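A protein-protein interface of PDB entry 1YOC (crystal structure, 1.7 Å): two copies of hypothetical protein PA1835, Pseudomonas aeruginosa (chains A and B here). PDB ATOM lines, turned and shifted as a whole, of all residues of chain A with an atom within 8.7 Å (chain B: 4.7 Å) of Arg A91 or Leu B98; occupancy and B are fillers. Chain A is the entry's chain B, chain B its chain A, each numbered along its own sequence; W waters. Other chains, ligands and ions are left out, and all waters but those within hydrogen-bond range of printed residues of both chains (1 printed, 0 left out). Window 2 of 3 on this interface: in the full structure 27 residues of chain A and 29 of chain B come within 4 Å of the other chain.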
ATOM      1  N   GLU A  71      -1.477 -27.670 -18.583  1.00  0.00           N
ATOM      2  CA  GLU A  71      -1.520 -28.166 -19.951  1.00  0.00           C
ATOM      3  C   GLU A  71      -2.882 -28.855 -20.211  1.00  0.00           C
ATOM      4  O   GLU A  71      -3.465 -28.719 -21.294  1.00  0.00           O
ATOM      5  CB  GLU A  71      -0.411 -29.188 -20.140  1.00  0.00           C
ATOM      6  CG  GLU A  71      -0.450 -29.860 -21.460  1.00  0.00           C
ATOM      7  CD  GLU A  71       0.339 -29.116 -22.507  1.00  0.00           C
ATOM      8  OE1 GLU A  71       0.467 -27.852 -22.419  1.00  0.00           O
ATOM      9  OE2 GLU A  71       0.811 -29.838 -23.429  1.00  0.00           O
ATOM     10  N   TRP A  88      -5.004 -27.078 -33.531  1.00  0.00           N
ATOM     11  CA  TRP A  88      -4.147 -26.362 -32.586  1.00  0.00           C
ATOM     12  C   TRP A  88      -2.965 -27.219 -32.171  1.00  0.00           C
ATOM     13  O   TRP A  88      -3.039 -28.461 -32.144  1.00  0.00           O
ATOM     14  CB  TRP A  88      -4.938 -26.001 -31.308  1.00  0.00           C
ATOM     15  CG  TRP A  88      -5.523 -27.216 -30.590  1.00  0.00           C
ATOM     16  CD1 TRP A  88      -6.678 -27.923 -30.932  1.00  0.00           C
ATOM     17  CD2 TRP A  88      -4.991 -27.888 -29.445  1.00  0.00           C
ATOM     18  NE1 TRP A  88      -6.870 -28.966 -30.084  1.00  0.00           N
ATOM     19  CE2 TRP A  88      -5.862 -28.981 -29.154  1.00  0.00           C
ATOM     20  CE3 TRP A  88      -3.872 -27.677 -28.622  1.00  0.00           C
ATOM     21  CZ2 TRP A  88      -5.637 -29.862 -28.079  1.00  0.00           C
ATOM     22  CZ3 TRP A  88      -3.652 -28.557 -27.544  1.00  0.00           C
ATOM     23  CH2 TRP A  88      -4.520 -29.628 -27.288  1.00  0.00           C
ATOM     24  N   ILE A  89      -1.880 -26.532 -31.824  1.00  0.00           N
ATOM     25  CA  ILE A  89      -0.685 -27.203 -31.344  1.00  0.00           C
ATOM     26  C   ILE A  89       0.015 -26.252 -30.358  1.00  0.00           C
ATOM     27  O   ILE A  89       0.182 -25.070 -30.655  1.00  0.00           O
ATOM     28  CB  ILE A  89       0.281 -27.591 -32.551  1.00  0.00           C
ATOM     29  CG1 ILE A  89       1.479 -28.362 -32.038  1.00  0.00           C
ATOM     30  CG2 ILE A  89       0.837 -26.386 -33.229  1.00  0.00           C
ATOM     31  CD1 ILE A  89       1.057 -29.426 -31.049  1.00  0.00           C
ATOM     32  N   PRO A  90       0.358 -26.749 -29.157  1.00  0.00           N
ATOM     33  CA  PRO A  90       1.044 -25.881 -28.191  1.00  0.00           C
ATOM     34  C   PRO A  90       2.438 -25.630 -28.741  1.00  0.00           C
ATOM     35  O   PRO A  90       3.092 -26.567 -29.234  1.00  0.00           O
ATOM     36  CB  PRO A  90       1.138 -26.736 -26.931  1.00  0.00           C
ATOM     37  CG  PRO A  90       0.000 -27.694 -27.051  1.00  0.00           C
ATOM     38  CD  PRO A  90       0.001 -28.040 -28.540  1.00  0.00           C
ATOM     39  N   ARG A  91       2.895 -24.389 -28.658  1.00  0.00           N
ATOM     40  CA  ARG A  91       4.243 -24.050 -29.148  1.00  0.00           C
ATOM     41  C   ARG A  91       5.117 -23.450 -28.077  1.00  0.00           C
ATOM     42  O   ARG A  91       6.325 -23.404 -28.232  1.00  0.00           O
ATOM     43  CB  ARG A  91       4.156 -23.075 -30.333  1.00  0.00           C
ATOM     44  CG  ARG A  91       3.724 -23.739 -31.603  1.00  0.00           C
ATOM     45  CD  ARG A  91       4.875 -24.631 -32.103  1.00  0.00           C
ATOM     46  NE  ARG A  91       4.520 -25.279 -33.358  1.00  0.00           N
ATOM     47  CZ  ARG A  91       4.950 -26.487 -33.742  1.00  0.00           C
ATOM     48  NH1 ARG A  91       5.773 -27.200 -32.972  1.00  0.00           N
ATOM     49  NH2 ARG A  91       4.526 -27.003 -34.892  1.00  0.00           N
ATOM     50  N   GLY A  92       4.522 -22.966 -26.994  1.00  0.00           N
ATOM     51  CA  GLY A  92       5.345 -22.432 -25.939  1.00  0.00           C
ATOM     52  C   GLY A  92       4.566 -22.329 -24.642  1.00  0.00           C
ATOM     53  O   GLY A  92       3.334 -22.422 -24.624  1.00  0.00           O
ATOM     54  N   MET A  93       5.289 -22.160 -23.549  1.00  0.00           N
ATOM     55  CA  MET A  93       4.626 -21.995 -22.253  1.00  0.00           C
ATOM     56  C   MET A  93       5.556 -21.240 -21.320  1.00  0.00           C
ATOM     57  O   MET A  93       6.772 -21.472 -21.324  1.00  0.00           O
ATOM     58  CB  MET A  93       4.275 -23.349 -21.605  1.00  0.00           C
ATOM     59  CG  MET A  93       3.783 -23.177 -20.138  1.00  0.00           C
ATOM     60  SD  MET A  93       3.317 -24.757 -19.362  1.00  0.00           S
ATOM     61  CE  MET A  93       4.935 -25.544 -19.214  1.00  0.00           C
ATOM     62  N   THR A  94       5.005 -20.275 -20.603  1.00  0.00           N
ATOM     63  CA  THR A  94       5.789 -19.573 -19.585  1.00  0.00           C
ATOM     64  C   THR A  94       5.030 -19.735 -18.285  1.00  0.00           C
ATOM     65  O   THR A  94       3.818 -19.536 -18.224  1.00  0.00           O
ATOM     66  CB  THR A  94       5.994 -18.058 -19.879  1.00  0.00           C
ATOM     67  OG1 THR A  94       6.818 -17.940 -21.050  1.00  0.00           O
ATOM     68  CG2 THR A  94       6.733 -17.358 -18.671  1.00  0.00           C
ATOM     69  N   GLY A 120      -3.602 -18.323 -35.822  1.00  0.00           N
ATOM     70  CA  GLY A 120      -2.373 -17.703 -35.347  1.00  0.00           C
ATOM     71  C   GLY A 120      -2.150 -18.125 -33.885  1.00  0.00           C
ATOM     72  O   GLY A 120      -2.717 -19.120 -33.425  1.00  0.00           O
ATOM     73  N   ASN A 121      -1.359 -17.347 -33.155  1.00  0.00           N
ATOM     74  CA  ASN A 121      -1.051 -17.650 -31.764  1.00  0.00           C
ATOM     75  C   ASN A 121      -2.094 -17.139 -30.815  1.00  0.00           C
ATOM     76  O   ASN A 121      -2.449 -15.966 -30.866  1.00  0.00           O
ATOM     77  CB  ASN A 121       0.302 -17.026 -31.400  1.00  0.00           C
ATOM     78  CG  ASN A 121       1.432 -17.695 -32.132  1.00  0.00           C
ATOM     79  OD1 ASN A 121       2.251 -17.047 -32.824  1.00  0.00           O
ATOM     80  ND2 ASN A 121       1.475 -18.998 -32.015  1.00  0.00           N
ATOM     81  N   LEU A 122      -2.599 -18.016 -29.970  1.00  0.00           N
ATOM     82  CA  LEU A 122      -3.573 -17.620 -28.941  1.00  0.00           C
ATOM     83  C   LEU A 122      -2.854 -17.964 -27.636  1.00  0.00           C
ATOM     84  O   LEU A 122      -2.306 -19.077 -27.495  1.00  0.00           O
ATOM     85  CB  LEU A 122      -4.871 -18.444 -29.036  1.00  0.00           C
ATOM     86  CG  LEU A 122      -5.585 -18.486 -30.397  1.00  0.00           C
ATOM     87  CD1 LEU A 122      -6.974 -19.211 -30.240  1.00  0.00           C
ATOM     88  CD2 LEU A 122      -5.770 -17.071 -30.917  1.00  0.00           C
ATOM     89  N   GLU A 139       1.051 -19.324 -18.975  1.00  0.00           N
ATOM     90  CA  GLU A 139       0.461 -18.827 -20.215  1.00  0.00           C
ATOM     91  C   GLU A 139       0.966 -19.847 -21.243  1.00  0.00           C
ATOM     92  O   GLU A 139       2.155 -20.051 -21.350  1.00  0.00           O
ATOM     93  CB  GLU A 139       0.964 -17.421 -20.529  1.00  0.00           C
ATOM     94  CG  GLU A 139       0.165 -16.344 -19.784  1.00  0.00           C
ATOM     95  CD  GLU A 139       0.770 -14.947 -19.958  1.00  0.00           C
ATOM     96  OE1 GLU A 139       1.650 -14.773 -20.841  1.00  0.00           O
ATOM     97  OE2 GLU A 139       0.346 -14.046 -19.210  1.00  0.00           O
ATOM     98  N   ILE A 140       0.056 -20.537 -21.931  1.00  0.00           N
ATOM     99  CA  ILE A 140       0.423 -21.527 -22.927  1.00  0.00           C
ATOM    100  C   ILE A 140      -0.018 -20.966 -24.288  1.00  0.00           C
ATOM    101  O   ILE A 140      -1.182 -20.654 -24.502  1.00  0.00           O
ATOM    102  CB  ILE A 140      -0.271 -22.856 -22.636  1.00  0.00           C
ATOM    103  CG1 ILE A 140       0.206 -23.391 -21.274  1.00  0.00           C
ATOM    104  CG2 ILE A 140       0.050 -23.865 -23.779  1.00  0.00           C
ATOM    105  CD1 ILE A 140      -0.607 -24.617 -20.744  1.00  0.00           C
ATOM    106  N   THR A 141       0.955 -20.837 -25.182  1.00  0.00           N
ATOM    107  CA  THR A 141       0.722 -20.308 -26.508  1.00  0.00           C
ATOM    108  C   THR A 141       0.399 -21.450 -27.444  1.00  0.00           C
ATOM    109  O   THR A 141       1.198 -22.377 -27.616  1.00  0.00           O
ATOM    110  CB  THR A 141       1.961 -19.556 -27.015  1.00  0.00           C
ATOM    111  OG1 THR A 141       2.211 -18.453 -26.122  1.00  0.00           O
ATOM    112  CG2 THR A 141       1.716 -19.010 -28.425  1.00  0.00           C
ATOM    113  N   MET A 142      -0.809 -21.390 -27.986  1.00  0.00           N
ATOM    114  CA  MET A 142      -1.320 -22.373 -28.919  1.00  0.00           C
ATOM    115  C   MET A 142      -1.233 -21.796 -30.325  1.00  0.00           C
ATOM    116  O   MET A 142      -1.665 -20.652 -30.557  1.00  0.00           O
ATOM    117  CB  MET A 142      -2.801 -22.650 -28.636  1.00  0.00           C
ATOM    118  CG  MET A 142      -3.086 -23.104 -27.226  1.00  0.00           C
ATOM    119  SD  MET A 142      -2.177 -24.649 -26.835  1.00  0.00           S
ATOM    120  CE  MET A 142      -2.948 -25.087 -25.274  1.00  0.00           C
ATOM    121  N   TYR A 143      -0.649 -22.550 -31.264  1.00  0.00           N
ATOM    122  CA  TYR A 143      -0.625 -22.060 -32.650  1.00  0.00           C
ATOM    123  C   TYR A 143      -1.859 -22.691 -33.324  1.00  0.00           C
ATOM    124  O   TYR A 143      -1.985 -23.922 -33.389  1.00  0.00           O
ATOM    125  CB  TYR A 143       0.610 -22.493 -33.419  1.00  0.00           C
ATOM    126  CG  TYR A 143       0.574 -21.898 -34.817  1.00  0.00           C
ATOM    127  CD1 TYR A 143       0.784 -20.541 -35.005  1.00  0.00           C
ATOM    128  CD2 TYR A 143       0.301 -22.689 -35.945  1.00  0.00           C
ATOM    129  CE1 TYR A 143       0.736 -19.968 -36.303  1.00  0.00           C
ATOM    130  CE2 TYR A 143       0.240 -22.120 -37.238  1.00  0.00           C
ATOM    131  CZ  TYR A 143       0.469 -20.757 -37.398  1.00  0.00           C
ATOM    132  OH  TYR A 143       0.520 -20.142 -38.666  1.00  0.00           O
ATOM    133  N   VAL A 144      -2.765 -21.841 -33.805  1.00  0.00           N
ATOM    134  CA  VAL A 144      -4.018 -22.317 -34.369  1.00  0.00           C
ATOM    135  C   VAL A 144      -4.014 -22.025 -35.846  1.00  0.00           C
ATOM    136  O   VAL A 144      -3.671 -20.929 -36.265  1.00  0.00           O
ATOM    137  CB  VAL A 144      -5.230 -21.593 -33.699  1.00  0.00           C
ATOM    138  CG1 VAL A 144      -6.559 -22.034 -34.362  1.00  0.00           C
ATOM    139  CG2 VAL A 144      -5.246 -21.890 -32.198  1.00  0.00           C
ATOM    140  N   SER A 145      -4.391 -23.020 -36.631  1.00  0.00           N
ATOM    141  CA  SER A 145      -4.420 -22.841 -38.076  1.00  0.00           C
ATOM    142  C   SER A 145      -5.641 -23.515 -38.725  1.00  0.00           C
ATOM    143  O   SER A 145      -6.143 -24.523 -38.222  1.00  0.00           O
ATOM    144  CB  SER A 145      -3.142 -23.420 -38.668  1.00  0.00           C
ATOM    145  OG  SER A 145      -3.083 -24.819 -38.427  1.00  0.00           O
ATOM    146  N   VAL B  95       9.396 -22.378 -21.995  1.00  0.00           N
ATOM    147  CA  VAL B  95       9.751 -23.484 -22.905  1.00  0.00           C
ATOM    148  C   VAL B  95       9.155 -23.244 -24.286  1.00  0.00           C
ATOM    149  O   VAL B  95       8.191 -22.470 -24.458  1.00  0.00           O
ATOM    150  CB  VAL B  95       9.198 -24.885 -22.431  1.00  0.00           C
ATOM    151  CG1 VAL B  95       9.655 -25.176 -20.982  1.00  0.00           C
ATOM    152  CG2 VAL B  95       7.659 -24.890 -22.469  1.00  0.00           C
ATOM    153  N   GLU B  96       9.765 -23.901 -25.274  1.00  0.00           N
ATOM    154  CA  GLU B  96       9.312 -23.877 -26.667  1.00  0.00           C
ATOM    155  C   GLU B  96       9.186 -25.333 -27.137  1.00  0.00           C
ATOM    156  O   GLU B  96      10.080 -26.172 -26.862  1.00  0.00           O
ATOM    157  CB  GLU B  96      10.319 -23.187 -27.615  1.00  0.00           C
ATOM    158  CG  GLU B  96      10.394 -21.678 -27.467  1.00  0.00           C
ATOM    159  CD  GLU B  96      11.459 -21.265 -26.489  1.00  0.00           C
ATOM    160  OE1 GLU B  96      12.593 -21.805 -26.577  1.00  0.00           O
ATOM    161  OE2 GLU B  96      11.171 -20.402 -25.630  1.00  0.00           O
ATOM    162  N   TYR B  97       8.101 -25.653 -27.835  1.00  0.00           N
ATOM    163  CA  TYR B  97       7.910 -27.014 -28.349  1.00  0.00           C
ATOM    164  C   TYR B  97       8.253 -26.939 -29.838  1.00  0.00           C
ATOM    165  O   TYR B  97       7.497 -26.337 -30.630  1.00  0.00           O
ATOM    166  CB  TYR B  97       6.459 -27.447 -28.109  1.00  0.00           C
ATOM    167  CG  TYR B  97       6.129 -27.382 -26.605  1.00  0.00           C
ATOM    168  CD1 TYR B  97       6.772 -28.227 -25.716  1.00  0.00           C
ATOM    169  CD2 TYR B  97       5.135 -26.520 -26.108  1.00  0.00           C
ATOM    170  CE1 TYR B  97       6.443 -28.249 -24.361  1.00  0.00           C
ATOM    171  CE2 TYR B  97       4.789 -26.537 -24.739  1.00  0.00           C
ATOM    172  CZ  TYR B  97       5.455 -27.414 -23.890  1.00  0.00           C
ATOM    173  OH  TYR B  97       5.146 -27.487 -22.570  1.00  0.00           O
ATOM    174  N   LEU B  98       9.391 -27.544 -30.204  1.00  0.00           N
ATOM    175  CA  LEU B  98       9.909 -27.440 -31.564  1.00  0.00           C
ATOM    176  C   LEU B  98       9.476 -28.503 -32.511  1.00  0.00           C
ATOM    177  O   LEU B  98       9.286 -28.233 -33.703  1.00  0.00           O
ATOM    178  CB  LEU B  98      11.447 -27.413 -31.524  1.00  0.00           C
ATOM    179  CG  LEU B  98      11.999 -26.451 -30.465  1.00  0.00           C
ATOM    180  CD1 LEU B  98      13.496 -26.540 -30.523  1.00  0.00           C
ATOM    181  CD2 LEU B  98      11.489 -24.999 -30.652  1.00  0.00           C
ATOM    182  N   ALA B  99       9.298 -29.713 -31.997  1.00  0.00           N
ATOM    183  CA  ALA B  99       8.909 -30.850 -32.834  1.00  0.00           C
ATOM    184  C   ALA B  99       8.310 -31.909 -31.961  1.00  0.00           C
ATOM    185  O   ALA B  99       8.495 -31.884 -30.748  1.00  0.00           O
ATOM    186  CB  ALA B  99      10.158 -31.424 -33.561  1.00  0.00           C
ATOM    187  N   PRO B 134      16.967 -31.559 -31.881  1.00  0.00           N
ATOM    188  CA  PRO B 134      16.234 -30.791 -30.868  1.00  0.00           C
ATOM    189  C   PRO B 134      14.723 -30.798 -31.057  1.00  0.00           C
ATOM    190  O   PRO B 134      14.236 -30.504 -32.153  1.00  0.00           O
ATOM    191  CB  PRO B 134      16.859 -29.401 -30.949  1.00  0.00           C
ATOM    192  CG  PRO B 134      17.235 -29.272 -32.480  1.00  0.00           C
ATOM    193  CD  PRO B 134      17.721 -30.699 -32.832  1.00  0.00           C
ATOM    194  N   VAL B 135      13.973 -31.126 -29.993  1.00  0.00           N
ATOM    195  CA  VAL B 135      12.511 -31.127 -30.114  1.00  0.00           C
ATOM    196  C   VAL B 135      11.893 -30.165 -29.114  1.00  0.00           C
ATOM    197  O   VAL B 135      10.693 -29.878 -29.177  1.00  0.00           O
ATOM    198  CB  VAL B 135      11.875 -32.525 -29.819  1.00  0.00           C
ATOM    199  CG1 VAL B 135      12.360 -33.567 -30.819  1.00  0.00           C
ATOM    200  CG2 VAL B 135      12.285 -33.026 -28.379  1.00  0.00           C
ATOM    201  N   PHE B 136      12.743 -29.634 -28.240  1.00  0.00           N
ATOM    202  CA  PHE B 136      12.260 -28.847 -27.116  1.00  0.00           C
ATOM    203  C   PHE B 136      13.395 -28.069 -26.499  1.00  0.00           C
ATOM    204  O   PHE B 136      14.539 -28.555 -26.427  1.00  0.00           O
ATOM    205  CB  PHE B 136      11.710 -29.852 -26.063  1.00  0.00           C
ATOM    206  CG  PHE B 136      11.481 -29.261 -24.669  1.00  0.00           C
ATOM    207  CD1 PHE B 136      10.191 -28.897 -24.252  1.00  0.00           C
ATOM    208  CD2 PHE B 136      12.534 -29.173 -23.753  1.00  0.00           C
ATOM    209  CE1 PHE B 136       9.953 -28.466 -22.925  1.00  0.00           C
ATOM    210  CE2 PHE B 136      12.304 -28.746 -22.444  1.00  0.00           C
ATOM    211  CZ  PHE B 136      10.988 -28.393 -22.032  1.00  0.00           C
ATOM    212  N   ARG B 137      13.079 -26.868 -26.045  1.00  0.00           N
ATOM    213  CA  ARG B 137      14.053 -26.039 -25.321  1.00  0.00           C
ATOM    214  C   ARG B 137      13.344 -25.365 -24.146  1.00  0.00           C
ATOM    215  O   ARG B 137      12.129 -25.083 -24.198  1.00  0.00           O
ATOM    216  CB  ARG B 137      14.684 -24.953 -26.223  1.00  0.00           C
ATOM    217  CG  ARG B 137      15.614 -25.578 -27.279  1.00  0.00           C
ATOM    218  CD  ARG B 137      16.252 -24.567 -28.245  1.00  0.00           C
ATOM    219  NE  ARG B 137      16.914 -23.501 -27.517  1.00  0.00           N
ATOM    220  CZ  ARG B 137      17.600 -22.515 -28.103  1.00  0.00           C
ATOM    221  NH1 ARG B 137      17.727 -22.461 -29.442  1.00  0.00           N
ATOM    222  NH2 ARG B 137      18.121 -21.558 -27.346  1.00  0.00           N
HETATM  223  O   HOH W   1       2.716 -26.355 -22.140  1.00  0.00           O
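Arg A91 touches just these residues of chain B: Glu B96, Tyr B97 and Leu B98. Of chain A, only Arg A91 (3.7 Å) comes within 4 Å of Leu B98. Ala B99 touches none of the printed residues of chain A. Printed residues of chain A within 4 Å of Tyr B97: Pro A90 (3.7 Å), Arg A91 (2.9 Å), Gly A92 (3.7 Å) and Met A93 (3.9 Å). Of the printed residues of chain A, Glu B96 touches Arg A91. Printed residues of chain B within 4 Å of Met A93: Val B95 and Tyr B97. Of the printed residues of chain A, Val B95 touches Gly A92 (3.2 Å) and Met A93 (2.9 Å). Tyr A143 touches none of the printed residues of chain B. Thr A141 touches none of the printed residues of chain B. The nearest residue of chain B that does not touch Arg A91 is Val B95 (4.3 Å).
Water W1 lies within hydrogen-bond range of the side-chain hydroxyl of Tyr B97, the side-chain carboxylate of Glu A71 and the side-chain sulfur of Met A93.
No position is printed for both chains. Of the 8 pairs that touch across the chains among the printed residues, none has its exchanged pair printed and touching as well.
Hydrophobic or aromatic side chains of chain B that line the printed part of chain A: Val B95 and Tyr B97. Hydrophobic or aromatic side chains of chain A within 4 Å of the printed part of chain B: Met A93. Among the printed residues, 8 pairs touch across the chains.
The backbone NH of Glu B96 sits at hydrogen-bond distance from the backbone carbonyl oxygen of Arg B137 (2.9 Å). O of Val B135 sits at hydrogen-bond distance from N of Leu B98. N of Arg A91 is in hydrogen-bond range of O of Thr A141 (2.8 Å). The backbone carbonyl oxygen of Gly A92 lies within hydrogen-bond range of the backbone NH of Thr A141 (2.9 Å).
Pro A90 touches Tyr B97. Arg A91 touches Glu B96 (O to CA, 3.4 Å). NH1 of Arg A91 touches O of Leu B98, 3.7 Å away. CA of Gly A92 touches O of Val B95, at 3.2 Å. N of Gly A92 touches CD2 of Tyr B97, at 3.7 Å. CE of Met A93 touches OH of Tyr B97, 3.9 Å away.
N of Val B95 sits at hydrogen-bond distance from O of Met A93, 2.9 Å away. The backbone carbonyl oxygen (O) of Arg A91 lies within hydrogen-bond range of the backbone NH (N) of Tyr B97.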
